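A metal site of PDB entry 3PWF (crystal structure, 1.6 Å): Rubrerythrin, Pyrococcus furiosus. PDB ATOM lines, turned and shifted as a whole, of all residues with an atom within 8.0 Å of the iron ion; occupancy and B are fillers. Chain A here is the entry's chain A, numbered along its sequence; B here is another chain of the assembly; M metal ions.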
ATOM      1  N   TYR A 108      15.320   2.419 -33.721  1.00  0.00           N
ATOM      2  CA  TYR A 108      14.707   1.728 -32.606  1.00  0.00           C
ATOM      3  C   TYR A 108      15.663   0.825 -31.882  1.00  0.00           C
ATOM      4  O   TYR A 108      15.819   0.792 -30.627  1.00  0.00           O
ATOM      5  CB  TYR A 108      13.511   0.875 -33.088  1.00  0.00           C
ATOM      6  CG  TYR A 108      12.275   1.643 -33.456  1.00  0.00           C
ATOM      7  CD1 TYR A 108      12.203   2.990 -33.331  1.00  0.00           C
ATOM      8  CD2 TYR A 108      11.179   0.955 -33.932  1.00  0.00           C
ATOM      9  CE1 TYR A 108      10.989   3.680 -33.626  1.00  0.00           C
ATOM     10  CE2 TYR A 108       9.960   1.612 -34.232  1.00  0.00           C
ATOM     11  CZ  TYR A 108       9.909   2.959 -34.000  1.00  0.00           C
ATOM     12  OH  TYR A 108       8.680   3.627 -34.390  1.00  0.00           O
ATOM     13  N   ILE A 140       9.326  -3.825 -21.312  1.00  0.00           N
ATOM     14  CA  ILE A 140       9.826  -3.744 -22.690  1.00  0.00           C
ATOM     15  C   ILE A 140       8.744  -3.220 -23.649  1.00  0.00           C
ATOM     16  O   ILE A 140       7.661  -3.778 -23.786  1.00  0.00           O
ATOM     17  CB  ILE A 140      10.286  -5.154 -23.195  1.00  0.00           C
ATOM     18  CG1 ILE A 140      11.267  -5.869 -22.210  1.00  0.00           C
ATOM     19  CG2 ILE A 140      10.882  -4.971 -24.583  1.00  0.00           C
ATOM     20  CD1 ILE A 140      12.665  -5.176 -22.022  1.00  0.00           C
ATOM     21  N   CYS A 141       9.086  -2.150 -24.372  1.00  0.00           N
ATOM     22  CA  CYS A 141       8.172  -1.648 -25.426  1.00  0.00           C
ATOM     23  C   CYS A 141       8.048  -2.640 -26.580  1.00  0.00           C
ATOM     24  O   CYS A 141       9.112  -3.094 -27.132  1.00  0.00           O
ATOM     25  CB  CYS A 141       8.661  -0.268 -25.980  1.00  0.00           C
ATOM     26  SG  CYS A 141       7.544   0.333 -27.299  1.00  0.00           S
ATOM     27  N   PRO A 142       6.858  -3.103 -26.920  1.00  0.00           N
ATOM     28  CA  PRO A 142       6.714  -4.080 -28.000  1.00  0.00           C
ATOM     29  C   PRO A 142       6.851  -3.545 -29.385  1.00  0.00           C
ATOM     30  O   PRO A 142       6.898  -4.368 -30.364  1.00  0.00           O
ATOM     31  CB  PRO A 142       5.256  -4.622 -27.777  1.00  0.00           C
ATOM     32  CG  PRO A 142       4.536  -3.354 -27.305  1.00  0.00           C
ATOM     33  CD  PRO A 142       5.539  -2.765 -26.283  1.00  0.00           C
ATOM     34  N   ILE A 143       6.964  -2.222 -29.513  1.00  0.00           N
ATOM     35  CA  ILE A 143       7.178  -1.599 -30.846  1.00  0.00           C
ATOM     36  C   ILE A 143       8.699  -1.436 -31.154  1.00  0.00           C
ATOM     37  O   ILE A 143       9.159  -1.687 -32.292  1.00  0.00           O
ATOM     38  CB  ILE A 143       6.504  -0.277 -30.839  1.00  0.00           C
ATOM     39  CG1 ILE A 143       4.977  -0.446 -30.439  1.00  0.00           C
ATOM     40  CG2 ILE A 143       6.667   0.400 -32.141  1.00  0.00           C
ATOM     41  CD1 ILE A 143       4.267  -1.427 -31.307  1.00  0.00           C
ATOM     42  N   CYS A 144       9.467  -0.948 -30.181  1.00  0.00           N
ATOM     43  CA  CYS A 144      10.848  -0.528 -30.439  1.00  0.00           C
ATOM     44  C   CYS A 144      11.811  -1.225 -29.536  1.00  0.00           C
ATOM     45  O   CYS A 144      13.085  -1.102 -29.763  1.00  0.00           O
ATOM     46  CB  CYS A 144      11.096   0.990 -30.429  1.00  0.00           C
ATOM     47  SG  CYS A 144      10.919   1.632 -28.715  1.00  0.00           S
ATOM     48  N   GLY A 145      11.351  -1.937 -28.487  1.00  0.00           N
ATOM     49  CA  GLY A 145      12.328  -2.582 -27.620  1.00  0.00           C
ATOM     50  C   GLY A 145      12.986  -1.708 -26.558  1.00  0.00           C
ATOM     51  O   GLY A 145      13.822  -2.185 -25.812  1.00  0.00           O
ATOM     52  N   TYR A 146      12.477  -0.476 -26.420  1.00  0.00           N
ATOM     53  CA  TYR A 146      12.852   0.356 -25.269  1.00  0.00           C
ATOM     54  C   TYR A 146      12.685  -0.462 -24.016  1.00  0.00           C
ATOM     55  O   TYR A 146      11.704  -1.207 -23.847  1.00  0.00           O
ATOM     56  CB  TYR A 146      11.916   1.640 -25.224  1.00  0.00           C
ATOM     57  CG  TYR A 146      12.051   2.408 -23.895  1.00  0.00           C
ATOM     58  CD1 TYR A 146      11.029   2.234 -22.934  1.00  0.00           C
ATOM     59  CD2 TYR A 146      13.162   3.205 -23.618  1.00  0.00           C
ATOM     60  CE1 TYR A 146      11.124   2.861 -21.718  1.00  0.00           C
ATOM     61  CE2 TYR A 146      13.266   3.852 -22.442  1.00  0.00           C
ATOM     62  CZ  TYR A 146      12.211   3.693 -21.506  1.00  0.00           C
ATOM     63  OH  TYR A 146      12.354   4.331 -20.268  1.00  0.00           O
ATOM     64  N   THR A 147      13.641  -0.302 -23.090  1.00  0.00           N
ATOM     65  CA  THR A 147      13.749  -1.207 -21.930  1.00  0.00           C
ATOM     66  C   THR A 147      13.899  -0.305 -20.690  1.00  0.00           C
ATOM     67  O   THR A 147      14.738   0.627 -20.627  1.00  0.00           O
ATOM     68  CB  THR A 147      15.023  -2.019 -22.091  1.00  0.00           C
ATOM     69  OG1 THR A 147      14.907  -2.860 -23.259  1.00  0.00           O
ATOM     70  CG2 THR A 147      15.316  -2.930 -20.889  1.00  0.00           C
ATOM     71  N   TYR A 155       4.859   7.071 -21.474  1.00  0.00           N
ATOM     72  CA  TYR A 155       4.881   6.867 -22.905  1.00  0.00           C
ATOM     73  C   TYR A 155       6.355   6.570 -23.249  1.00  0.00           C
ATOM     74  O   TYR A 155       7.292   7.093 -22.676  1.00  0.00           O
ATOM     75  CB  TYR A 155       4.469   8.134 -23.637  1.00  0.00           C
ATOM     76  CG  TYR A 155       2.975   8.451 -23.390  1.00  0.00           C
ATOM     77  CD1 TYR A 155       1.995   7.696 -24.044  1.00  0.00           C
ATOM     78  CD2 TYR A 155       2.658   9.318 -22.375  1.00  0.00           C
ATOM     79  CE1 TYR A 155       0.639   7.885 -23.734  1.00  0.00           C
ATOM     80  CE2 TYR A 155       1.254   9.550 -22.093  1.00  0.00           C
ATOM     81  CZ  TYR A 155       0.322   8.804 -22.783  1.00  0.00           C
ATOM     82  OH  TYR A 155      -1.017   9.013 -22.435  1.00  0.00           O
ATOM     83  N   CYS A 156       6.518   5.596 -24.195  1.00  0.00           N
ATOM     84  CA  CYS A 156       7.868   5.249 -24.649  1.00  0.00           C
ATOM     85  C   CYS A 156       8.529   6.513 -25.233  1.00  0.00           C
ATOM     86  O   CYS A 156       7.986   7.208 -26.101  1.00  0.00           O
ATOM     87  CB  CYS A 156       7.618   4.231 -25.731  1.00  0.00           C
ATOM     88  SG  CYS A 156       9.374   3.778 -26.450  1.00  0.00           S
ATOM     89  N   PRO A 157       9.803   6.779 -24.824  1.00  0.00           N
ATOM     90  CA  PRO A 157      10.411   8.048 -25.327  1.00  0.00           C
ATOM     91  C   PRO A 157      10.907   7.938 -26.775  1.00  0.00           C
ATOM     92  O   PRO A 157      11.186   8.967 -27.416  1.00  0.00           O
ATOM     93  CB  PRO A 157      11.594   8.288 -24.368  1.00  0.00           C
ATOM     94  CG  PRO A 157      11.942   6.887 -23.910  1.00  0.00           C
ATOM     95  CD  PRO A 157      10.553   6.153 -23.746  1.00  0.00           C
ATOM     96  N   VAL A 158      10.887   6.689 -27.291  1.00  0.00           N
ATOM     97  CA  VAL A 158      11.377   6.546 -28.672  1.00  0.00           C
ATOM     98  C   VAL A 158      10.230   6.545 -29.612  1.00  0.00           C
ATOM     99  O   VAL A 158      10.302   7.301 -30.635  1.00  0.00           O
ATOM    100  CB  VAL A 158      12.257   5.224 -28.772  1.00  0.00           C
ATOM    101  CG1 VAL A 158      12.552   5.021 -30.319  1.00  0.00           C
ATOM    102  CG2 VAL A 158      13.510   5.322 -27.921  1.00  0.00           C
ATOM    103  N   CYS A 159       9.191   5.767 -29.338  1.00  0.00           N
ATOM    104  CA  CYS A 159       8.104   5.686 -30.328  1.00  0.00           C
ATOM    105  C   CYS A 159       6.776   6.187 -29.816  1.00  0.00           C
ATOM    106  O   CYS A 159       5.799   6.230 -30.591  1.00  0.00           O
ATOM    107  CB  CYS A 159       7.957   4.210 -30.771  1.00  0.00           C
ATOM    108  SG  CYS A 159       7.227   3.095 -29.513  1.00  0.00           S
ATOM    109  N   GLY A 160       6.704   6.570 -28.543  1.00  0.00           N
ATOM    110  CA  GLY A 160       5.491   7.132 -27.942  1.00  0.00           C
ATOM    111  C   GLY A 160       4.387   6.141 -27.560  1.00  0.00           C
ATOM    112  O   GLY A 160       3.295   6.539 -27.101  1.00  0.00           O
ATOM    113  N   ALA A 161       4.616   4.839 -27.692  1.00  0.00           N
ATOM    114  CA  ALA A 161       3.626   3.831 -27.195  1.00  0.00           C
ATOM    115  C   ALA A 161       3.343   4.019 -25.729  1.00  0.00           C
ATOM    116  O   ALA A 161       4.212   4.282 -24.885  1.00  0.00           O
ATOM    117  CB  ALA A 161       4.197   2.330 -27.317  1.00  0.00           C
ATOM    118  N   PRO A 162       2.069   3.789 -25.346  1.00  0.00           N
ATOM    119  CA  PRO A 162       1.690   3.980 -23.941  1.00  0.00           C
ATOM    120  C   PRO A 162       2.220   2.837 -23.116  1.00  0.00           C
ATOM    121  O   PRO A 162       2.257   1.647 -23.510  1.00  0.00           O
ATOM    122  CB  PRO A 162       0.139   3.905 -23.984  1.00  0.00           C
ATOM    123  CG  PRO A 162      -0.208   3.158 -25.230  1.00  0.00           C
ATOM    124  CD  PRO A 162       0.940   3.461 -26.248  1.00  0.00           C
ATOM    125  N   PHE A 166       3.404  -1.944 -22.645  1.00  0.00           N
ATOM    126  CA  PHE A 166       4.731  -2.566 -22.373  1.00  0.00           C
ATOM    127  C   PHE A 166       4.609  -3.967 -21.828  1.00  0.00           C
ATOM    128  O   PHE A 166       3.671  -4.309 -20.987  1.00  0.00           O
ATOM    129  CB  PHE A 166       5.567  -1.747 -21.383  1.00  0.00           C
ATOM    130  CG  PHE A 166       5.895  -0.323 -21.839  1.00  0.00           C
ATOM    131  CD1 PHE A 166       5.650   0.132 -23.131  1.00  0.00           C
ATOM    132  CD2 PHE A 166       6.418   0.539 -20.882  1.00  0.00           C
ATOM    133  CE1 PHE A 166       5.983   1.436 -23.547  1.00  0.00           C
ATOM    134  CE2 PHE A 166       6.769   1.932 -21.230  1.00  0.00           C
ATOM    135  CZ  PHE A 166       6.582   2.391 -22.580  1.00  0.00           C
ATOM    136  N   VAL B  53      11.837  -8.069 -30.481  1.00  0.00           N
ATOM    137  CA  VAL B  53      11.233  -6.959 -31.087  1.00  0.00           C
ATOM    138  C   VAL B  53      12.107  -6.358 -32.224  1.00  0.00           C
ATOM    139  O   VAL B  53      11.614  -6.097 -33.327  1.00  0.00           O
ATOM    140  CB  VAL B  53      10.885  -5.823 -30.103  1.00  0.00           C
ATOM    141  CG1 VAL B  53      10.370  -4.556 -30.746  1.00  0.00           C
ATOM    142  CG2 VAL B  53       9.878  -6.341 -28.999  1.00  0.00           C
HETATM  143 FE    FE M   1       8.773   2.193 -28.045  1.00  0.00          FE
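Of the 19 residues printed, 4 come within 4 Å of the iron ion.
The nearest printed residue that does not touch the iron ion is Tyr 146 (4.3 Å).
N of Ala 161 lies close to SG of Cys 159, at 3.6 Å.
SG of Cys 144 sits close to N of Tyr 146.
The backbone NH of Cys 156 sits at hydrogen-bond distance from the backbone carbonyl oxygen of Ala 161 (2.7 Å).
The side-chain sulfur of Cys 156 sits close to the backbone NH of Val 158 (3.4 Å).
The backbone carbonyl oxygen (O) of Tyr 146 sits at hydrogen-bond distance from the backbone NH (N) of Cys 141 (2.8 Å).
SG of Cys 141 sits close to N of Ile 143 (3.4 Å).
The iron ion is bound by the side-chain sulfur of Cys 159, the side-chain sulfur of Cys 144, the side-chain sulfur of Cys 156 and the side-chain sulfur of Cys 141.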
